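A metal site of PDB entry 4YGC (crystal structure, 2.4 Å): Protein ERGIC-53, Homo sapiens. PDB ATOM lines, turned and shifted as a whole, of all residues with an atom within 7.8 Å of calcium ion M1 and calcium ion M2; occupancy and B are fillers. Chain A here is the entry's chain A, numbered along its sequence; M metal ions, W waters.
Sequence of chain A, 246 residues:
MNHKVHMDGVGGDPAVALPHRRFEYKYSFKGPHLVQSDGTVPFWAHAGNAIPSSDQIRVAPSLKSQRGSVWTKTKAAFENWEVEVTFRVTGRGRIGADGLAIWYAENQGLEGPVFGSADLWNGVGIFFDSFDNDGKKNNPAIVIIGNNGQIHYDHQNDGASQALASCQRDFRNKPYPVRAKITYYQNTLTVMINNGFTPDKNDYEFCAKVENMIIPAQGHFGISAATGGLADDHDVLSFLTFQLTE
The nearest printed residue that does not touch calcium ion M2 is Lys 136 (4.4 Å).
Four residues have an atom within 4 Å of calcium ion M1: Asp 129, Phe 131, Asn 133 and Asp 158.
Calcium ion M2 is bound by the side-chain carboxylate (OD2) of Asp 158, the side-chain amide oxygen (OD1) of Asn 138, the side-chain carboxylate (OD1) of Asp 132, the side-chain amide oxygen (OD1) of Asn 139 and the side-chain carboxylate (OD1) of Asp 134.
Calcium ion M2 has five donor atoms within binding distance.
Water W1 bridges the side-chain hydroxyl of Tyr 153 (3.0 Å) and the backbone carbonyl oxygen of His 155 (3.0 Å).
The backbone carbonyl oxygen (O) of Asp 129 sits at hydrogen-bond distance from the side-chain amide nitrogen (ND2) of Asn 139, 3.3 Å away.
The backbone NH of Asp 129 lies within hydrogen-bond range of the backbone carbonyl oxygen of Ala 141 (2.8 Å).
The backbone carbonyl oxygen (O) of Phe 131 sits close to the side-chain amide nitrogen (ND2) of Asn 139 (3.5 Å).
The side-chain carboxylate (OD2) of Asp 132 is in hydrogen-bond range of the backbone NH (N) of Lys 136 (3.0 Å).
The side-chain carboxylate (OD1) of Asp 132 lies close to the backbone NH (N) of Gly 135, at 3.3 Å.
The side-chain carboxylate (OD2) of Asp 132 is in hydrogen-bond range of the backbone NH (N) of Lys 137, at 2.6 Å.
The backbone NH (N) of Asn 139 lies close to the side-chain amide nitrogen (NE2) of Gln 168.
N of Asp 134 is in hydrogen-bond range of O of Gln 156 (3.3 Å).
Calcium ion M1 is bound by OD1 of Asp 158 (2.2 Å), OD1 of Asp 129 (2.3 Å), OD1 of Asn 133 (2.3 Å), water W2 (2.3 Å), water W1 (2.3 Å), O of Phe 131 (2.4 Å) and OD2 of Asp 129 (2.5 Å).
Calcium ion M1 has seven donor atoms within binding distance.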
ATOM      1  N   GLY A  96      15.893  21.738   5.752  1.00  0.00           N
ATOM      2  CA  GLY A  96      15.295  20.732   4.884  1.00  0.00           C
ATOM      3  C   GLY A  96      14.904  19.468   5.664  1.00  0.00           C
ATOM      4  O   GLY A  96      15.168  19.367   6.846  1.00  0.00           O
ATOM      5  N   ALA A  97      14.259  18.533   4.983  1.00  0.00           N
ATOM      6  CA  ALA A  97      13.664  17.364   5.606  1.00  0.00           C
ATOM      7  C   ALA A  97      13.588  16.194   4.621  1.00  0.00           C
ATOM      8  O   ALA A  97      13.509  16.462   3.408  1.00  0.00           O
ATOM      9  CB  ALA A  97      12.283  17.717   6.096  1.00  0.00           C
ATOM     10  N   ASP A  98      13.580  14.920   5.074  1.00  0.00           N
ATOM     11  CA  ASP A  98      13.733  14.508   6.455  1.00  0.00           C
ATOM     12  C   ASP A  98      15.104  13.970   6.725  1.00  0.00           C
ATOM     13  O   ASP A  98      15.654  14.147   7.814  1.00  0.00           O
ATOM     14  CB  ASP A  98      12.716  13.418   6.837  1.00  0.00           C
ATOM     15  CG  ASP A  98      11.416  13.989   7.300  1.00  0.00           C
ATOM     16  OD1 ASP A  98      10.411  13.868   6.591  1.00  0.00           O
ATOM     17  OD2 ASP A  98      11.425  14.712   8.303  1.00  0.00           O
ATOM     18  N   GLY A  99      15.681  13.335   5.707  1.00  0.00           N
ATOM     19  CA  GLY A  99      17.037  12.853   5.803  1.00  0.00           C
ATOM     20  C   GLY A  99      17.157  11.531   5.127  1.00  0.00           C
ATOM     21  O   GLY A  99      16.282  11.079   4.419  1.00  0.00           O
ATOM     22  N   PHE A 115      12.555   6.993   7.670  1.00  0.00           N
ATOM     23  CA  PHE A 115      13.301   7.544   6.554  1.00  0.00           C
ATOM     24  C   PHE A 115      13.052   6.730   5.323  1.00  0.00           C
ATOM     25  O   PHE A 115      13.999   6.423   4.556  1.00  0.00           O
ATOM     26  CB  PHE A 115      14.776   7.599   6.906  1.00  0.00           C
ATOM     27  CG  PHE A 115      15.110   8.554   8.007  1.00  0.00           C
ATOM     28  CD1 PHE A 115      15.247   9.892   7.735  1.00  0.00           C
ATOM     29  CD2 PHE A 115      15.234   8.120   9.295  1.00  0.00           C
ATOM     30  CE1 PHE A 115      15.509  10.804   8.745  1.00  0.00           C
ATOM     31  CE2 PHE A 115      15.531   9.025  10.314  1.00  0.00           C
ATOM     32  CZ  PHE A 115      15.661  10.367  10.031  1.00  0.00           C
ATOM     33  N   PHE A 128      20.835  10.070   8.994  1.00  0.00           N
ATOM     34  CA  PHE A 128      21.340  11.428   8.689  1.00  0.00           C
ATOM     35  C   PHE A 128      20.097  12.274   8.689  1.00  0.00           C
ATOM     36  O   PHE A 128      19.373  12.295   7.704  1.00  0.00           O
ATOM     37  CB  PHE A 128      22.054  11.454   7.336  1.00  0.00           C
ATOM     38  CG  PHE A 128      23.267  10.602   7.308  1.00  0.00           C
ATOM     39  CD1 PHE A 128      24.517  11.167   7.263  1.00  0.00           C
ATOM     40  CD2 PHE A 128      23.158   9.215   7.408  1.00  0.00           C
ATOM     41  CE1 PHE A 128      25.644  10.380   7.280  1.00  0.00           C
ATOM     42  CE2 PHE A 128      24.276   8.417   7.407  1.00  0.00           C
ATOM     43  CZ  PHE A 128      25.528   8.998   7.368  1.00  0.00           C
ATOM     44  N   ASP A 129      19.832  12.887   9.831  1.00  0.00           N
ATOM     45  CA  ASP A 129      18.523  13.501  10.117  1.00  0.00           C
ATOM     46  C   ASP A 129      18.617  15.002   9.898  1.00  0.00           C
ATOM     47  O   ASP A 129      19.289  15.681  10.660  1.00  0.00           O
ATOM     48  CB  ASP A 129      18.089  13.187  11.545  1.00  0.00           C
ATOM     49  CG  ASP A 129      16.650  13.607  11.857  1.00  0.00           C
ATOM     50  OD1 ASP A 129      15.983  14.298  11.041  1.00  0.00           O
ATOM     51  OD2 ASP A 129      16.153  13.247  12.928  1.00  0.00           O
ATOM     52  N   SER A 130      17.974  15.504   8.855  1.00  0.00           N
ATOM     53  CA  SER A 130      18.060  16.920   8.498  1.00  0.00           C
ATOM     54  C   SER A 130      17.181  17.808   9.346  1.00  0.00           C
ATOM     55  O   SER A 130      17.503  18.964   9.562  1.00  0.00           O
ATOM     56  CB  SER A 130      17.540  17.126   7.099  1.00  0.00           C
ATOM     57  OG  SER A 130      18.116  16.271   6.144  1.00  0.00           O
ATOM     58  N   PHE A 131      16.013  17.293   9.737  1.00  0.00           N
ATOM     59  CA  PHE A 131      14.954  18.118  10.292  1.00  0.00           C
ATOM     60  C   PHE A 131      14.757  17.918  11.776  1.00  0.00           C
ATOM     61  O   PHE A 131      14.612  16.793  12.276  1.00  0.00           O
ATOM     62  CB  PHE A 131      13.642  17.845   9.576  1.00  0.00           C
ATOM     63  CG  PHE A 131      12.538  18.744  10.023  1.00  0.00           C
ATOM     64  CD1 PHE A 131      12.526  20.089   9.627  1.00  0.00           C
ATOM     65  CD2 PHE A 131      11.508  18.266  10.853  1.00  0.00           C
ATOM     66  CE1 PHE A 131      11.527  20.954  10.077  1.00  0.00           C
ATOM     67  CE2 PHE A 131      10.492  19.125  11.274  1.00  0.00           C
ATOM     68  CZ  PHE A 131      10.487  20.465  10.890  1.00  0.00           C
ATOM     69  N   ASP A 132      14.777  19.045  12.484  1.00  0.00           N
ATOM     70  CA  ASP A 132      14.749  19.115  13.933  1.00  0.00           C
ATOM     71  C   ASP A 132      13.299  18.988  14.445  1.00  0.00           C
ATOM     72  O   ASP A 132      12.677  19.960  14.814  1.00  0.00           O
ATOM     73  CB  ASP A 132      15.350  20.457  14.339  1.00  0.00           C
ATOM     74  CG  ASP A 132      15.562  20.580  15.822  1.00  0.00           C
ATOM     75  OD1 ASP A 132      15.626  19.559  16.512  1.00  0.00           O
ATOM     76  OD2 ASP A 132      15.721  21.738  16.263  1.00  0.00           O
ATOM     77  N   ASN A 133      12.789  17.765  14.458  1.00  0.00           N
ATOM     78  CA  ASN A 133      11.391  17.478  14.830  1.00  0.00           C
ATOM     79  C   ASN A 133      11.049  17.874  16.283  1.00  0.00           C
ATOM     80  O   ASN A 133       9.892  18.133  16.591  1.00  0.00           O
ATOM     81  CB  ASN A 133      11.093  15.984  14.622  1.00  0.00           C
ATOM     82  CG  ASN A 133      10.953  15.601  13.160  1.00  0.00           C
ATOM     83  OD1 ASN A 133      11.896  15.108  12.510  1.00  0.00           O
ATOM     84  ND2 ASN A 133       9.728  15.784  12.627  1.00  0.00           N
ATOM     85  N   ASP A 134      12.034  17.819  17.162  1.00  0.00           N
ATOM     86  CA  ASP A 134      11.865  18.203  18.563  1.00  0.00           C
ATOM     87  C   ASP A 134      12.254  19.669  18.880  1.00  0.00           C
ATOM     88  O   ASP A 134      12.147  20.085  20.012  1.00  0.00           O
ATOM     89  CB  ASP A 134      12.622  17.229  19.496  1.00  0.00           C
ATOM     90  CG  ASP A 134      14.084  17.099  19.176  1.00  0.00           C
ATOM     91  OD1 ASP A 134      14.559  17.794  18.225  1.00  0.00           O
ATOM     92  OD2 ASP A 134      14.793  16.315  19.845  1.00  0.00           O
ATOM     93  N   GLY A 135      12.730  20.431  17.903  1.00  0.00           N
ATOM     94  CA  GLY A 135      13.081  21.823  18.120  1.00  0.00           C
ATOM     95  C   GLY A 135      14.211  22.111  19.080  1.00  0.00           C
ATOM     96  O   GLY A 135      14.221  23.144  19.713  1.00  0.00           O
ATOM     97  N   LYS A 136      15.154  21.198  19.210  1.00  0.00           N
ATOM     98  CA  LYS A 136      16.310  21.402  20.094  1.00  0.00           C
ATOM     99  C   LYS A 136      17.498  22.095  19.423  1.00  0.00           C
ATOM    100  O   LYS A 136      18.576  22.136  20.007  1.00  0.00           O
ATOM    101  CB  LYS A 136      16.773  20.053  20.647  1.00  0.00           C
ATOM    102  CG  LYS A 136      15.669  19.236  21.311  1.00  0.00           C
ATOM    103  CD  LYS A 136      15.500  19.433  22.771  1.00  0.00           C
ATOM    104  CE  LYS A 136      15.002  18.051  23.208  1.00  0.00           C
ATOM    105  NZ  LYS A 136      16.137  17.151  23.553  1.00  0.00           N
ATOM    106  N   LYS A 137      17.315  22.559  18.181  1.00  0.00           N
ATOM    107  CA  LYS A 137      18.384  23.248  17.424  1.00  0.00           C
ATOM    108  C   LYS A 137      19.697  22.424  17.386  1.00  0.00           C
ATOM    109  O   LYS A 137      20.789  22.936  17.574  1.00  0.00           O
ATOM    110  CB  LYS A 137      18.563  24.698  17.898  1.00  0.00           C
ATOM    111  CG  LYS A 137      17.489  25.596  17.288  1.00  0.00           C
ATOM    112  CD  LYS A 137      17.036  26.770  18.115  1.00  0.00           C
ATOM    113  CE  LYS A 137      15.663  27.279  17.628  1.00  0.00           C
ATOM    114  NZ  LYS A 137      15.626  28.756  17.387  1.00  0.00           N
ATOM    115  N   ASN A 138      19.556  21.122  17.151  1.00  0.00           N
ATOM    116  CA  ASN A 138      20.673  20.198  17.137  1.00  0.00           C
ATOM    117  C   ASN A 138      20.567  19.315  15.875  1.00  0.00           C
ATOM    118  O   ASN A 138      20.721  18.093  15.944  1.00  0.00           O
ATOM    119  CB  ASN A 138      20.622  19.329  18.405  1.00  0.00           C
ATOM    120  CG  ASN A 138      19.329  18.571  18.517  1.00  0.00           C
ATOM    121  OD1 ASN A 138      18.338  18.948  17.905  1.00  0.00           O
ATOM    122  ND2 ASN A 138      19.327  17.508  19.306  1.00  0.00           N
ATOM    123  N   ASN A 139      20.303  19.958  14.747  1.00  0.00           N
ATOM    124  CA  ASN A 139      20.293  19.309  13.446  1.00  0.00           C
ATOM    125  C   ASN A 139      21.006  20.169  12.426  1.00  0.00           C
ATOM    126  O   ASN A 139      21.045  21.369  12.610  1.00  0.00           O
ATOM    127  CB  ASN A 139      18.860  19.077  13.018  1.00  0.00           C
ATOM    128  CG  ASN A 139      18.172  18.075  13.907  1.00  0.00           C
ATOM    129  OD1 ASN A 139      17.854  18.384  15.052  1.00  0.00           O
ATOM    130  ND2 ASN A 139      17.919  16.878  13.383  1.00  0.00           N
ATOM    131  N   PRO A 140      21.516  19.589  11.306  1.00  0.00           N
ATOM    132  CA  PRO A 140      21.440  18.171  10.961  1.00  0.00           C
ATOM    133  C   PRO A 140      22.284  17.352  11.880  1.00  0.00           C
ATOM    134  O   PRO A 140      23.243  17.844  12.428  1.00  0.00           O
ATOM    135  CB  PRO A 140      22.010  18.124   9.526  1.00  0.00           C
ATOM    136  CG  PRO A 140      21.724  19.475   8.962  1.00  0.00           C
ATOM    137  CD  PRO A 140      21.948  20.400  10.144  1.00  0.00           C
ATOM    138  N   ALA A 141      21.910  16.087  12.055  1.00  0.00           N
ATOM    139  CA  ALA A 141      22.563  15.215  13.035  1.00  0.00           C
ATOM    140  C   ALA A 141      22.715  13.836  12.458  1.00  0.00           C
ATOM    141  O   ALA A 141      21.926  13.431  11.620  1.00  0.00           O
ATOM    142  CB  ALA A 141      21.703  15.117  14.289  1.00  0.00           C
ATOM    143  N   TYR A 153      10.795   3.493  16.093  1.00  0.00           N
ATOM    144  CA  TYR A 153      11.622   4.712  15.951  1.00  0.00           C
ATOM    145  C   TYR A 153      10.836   5.935  16.414  1.00  0.00           C
ATOM    146  O   TYR A 153       9.692   6.173  15.972  1.00  0.00           O
ATOM    147  CB  TYR A 153      12.070   4.899  14.508  1.00  0.00           C
ATOM    148  CG  TYR A 153      12.689   6.241  14.218  1.00  0.00           C
ATOM    149  CD1 TYR A 153      13.855   6.638  14.863  1.00  0.00           C
ATOM    150  CD2 TYR A 153      12.105   7.126  13.298  1.00  0.00           C
ATOM    151  CE1 TYR A 153      14.421   7.878  14.616  1.00  0.00           C
ATOM    152  CE2 TYR A 153      12.708   8.342  12.995  1.00  0.00           C
ATOM    153  CZ  TYR A 153      13.852   8.711  13.652  1.00  0.00           C
ATOM    154  OH  TYR A 153      14.417   9.936  13.399  1.00  0.00           O
ATOM    155  N   ASP A 154      11.443   6.714  17.296  1.00  0.00           N
ATOM    156  CA  ASP A 154      10.869   7.923  17.855  1.00  0.00           C
ATOM    157  C   ASP A 154      11.055   9.139  16.918  1.00  0.00           C
ATOM    158  O   ASP A 154      11.875  10.033  17.162  1.00  0.00           O
ATOM    159  CB  ASP A 154      11.530   8.217  19.227  1.00  0.00           C
ATOM    160  CG  ASP A 154      10.743   9.239  20.067  1.00  0.00           C
ATOM    161  OD1 ASP A 154       9.714   9.783  19.589  1.00  0.00           O
ATOM    162  OD2 ASP A 154      11.197   9.547  21.192  1.00  0.00           O
ATOM    163  N   HIS A 155      10.315   9.137  15.823  1.00  0.00           N
ATOM    164  CA  HIS A 155      10.395  10.195  14.819  1.00  0.00           C
ATOM    165  C   HIS A 155      10.308  11.616  15.372  1.00  0.00           C
ATOM    166  O   HIS A 155      11.154  12.469  15.079  1.00  0.00           O
ATOM    167  CB  HIS A 155       9.300  10.021  13.759  1.00  0.00           C
ATOM    168  CG  HIS A 155       9.471  10.912  12.566  1.00  0.00           C
ATOM    169  ND1 HIS A 155      10.439  10.713  11.596  1.00  0.00           N
ATOM    170  CD2 HIS A 155       8.825  12.056  12.210  1.00  0.00           C
ATOM    171  CE1 HIS A 155      10.365  11.684  10.696  1.00  0.00           C
ATOM    172  NE2 HIS A 155       9.392  12.508  11.042  1.00  0.00           N
ATOM    173  N   GLN A 156       9.333  11.873  16.189  1.00  0.00           N
ATOM    174  CA  GLN A 156       9.089  13.247  16.662  1.00  0.00           C
ATOM    175  C   GLN A 156      10.212  13.819  17.587  1.00  0.00           C
ATOM    176  O   GLN A 156      10.308  15.025  17.762  1.00  0.00           O
ATOM    177  CB  GLN A 156       7.656  13.353  17.227  1.00  0.00           C
ATOM    178  CG  GLN A 156       7.565  13.259  18.734  1.00  0.00           C
ATOM    179  CD  GLN A 156       6.276  12.661  19.290  1.00  0.00           C
ATOM    180  OE1 GLN A 156       6.090  12.576  20.525  1.00  0.00           O
ATOM    181  NE2 GLN A 156       5.414  12.169  18.388  1.00  0.00           N
ATOM    182  N   ASN A 157      11.071  12.946  18.137  1.00  0.00           N
ATOM    183  CA  ASN A 157      12.209  13.392  18.955  1.00  0.00           C
ATOM    184  C   ASN A 157      13.555  13.099  18.314  1.00  0.00           C
ATOM    185  O   ASN A 157      14.592  13.063  19.001  1.00  0.00           O
ATOM    186  CB  ASN A 157      12.136  12.764  20.342  1.00  0.00           C
ATOM    187  CG  ASN A 157      10.852  13.168  21.067  1.00  0.00           C
ATOM    188  OD1 ASN A 157      10.673  14.330  21.430  1.00  0.00           O
ATOM    189  ND2 ASN A 157       9.964  12.226  21.235  1.00  0.00           N
ATOM    190  N   ASP A 158      13.533  12.882  16.988  1.00  0.00           N
ATOM    191  CA  ASP A 158      14.748  12.567  16.215  1.00  0.00           C
ATOM    192  C   ASP A 158      15.510  11.392  16.846  1.00  0.00           C
ATOM    193  O   ASP A 158      16.723  11.388  16.833  1.00  0.00           O
ATOM    194  CB  ASP A 158      15.699  13.806  16.089  1.00  0.00           C
ATOM    195  CG  ASP A 158      15.057  15.030  15.407  1.00  0.00           C
ATOM    196  OD1 ASP A 158      14.247  14.861  14.457  1.00  0.00           O
ATOM    197  OD2 ASP A 158      15.337  16.134  15.877  1.00  0.00           O
ATOM    198  N   GLY A 159      14.778  10.409  17.367  1.00  0.00           N
ATOM    199  CA  GLY A 159      15.349   9.241  18.005  1.00  0.00           C
ATOM    200  C   GLY A 159      16.332   9.505  19.112  1.00  0.00           C
ATOM    201  O   GLY A 159      17.142   8.642  19.451  1.00  0.00           O
ATOM    202  N   ALA A 160      16.276  10.693  19.707  1.00  0.00           N
ATOM    203  CA  ALA A 160      17.299  11.086  20.662  1.00  0.00           C
ATOM    204  C   ALA A 160      17.457  10.113  21.864  1.00  0.00           C
ATOM    205  O   ALA A 160      18.554   9.956  22.377  1.00  0.00           O
ATOM    206  CB  ALA A 160      17.045  12.508  21.155  1.00  0.00           C
ATOM    207  N   GLN A 168      26.703  16.090  15.521  1.00  0.00           N
ATOM    208  CA  GLN A 168      26.136  17.199  14.770  1.00  0.00           C
ATOM    209  C   GLN A 168      27.005  17.433  13.547  1.00  0.00           C
ATOM    210  O   GLN A 168      28.194  17.621  13.652  1.00  0.00           O
ATOM    211  CB  GLN A 168      26.025  18.443  15.661  1.00  0.00           C
ATOM    212  CG  GLN A 168      24.778  18.429  16.567  1.00  0.00           C
ATOM    213  CD  GLN A 168      24.140  19.798  16.664  1.00  0.00           C
ATOM    214  OE1 GLN A 168      24.133  20.445  17.717  1.00  0.00           O
ATOM    215  NE2 GLN A 168      23.631  20.263  15.547  1.00  0.00           N
HETATM  216 CA    CA M   1      14.118  14.483  12.305  1.00  0.00          CA
HETATM  217 CA    CA M   2      16.748  17.478  17.044  1.00  0.00          CA
HETATM  218  O   HOH W   1      13.020  12.447  12.718  1.00  0.00           O
HETATM  219  O   HOH W   2      13.579  14.089  10.079  1.00  0.00           O
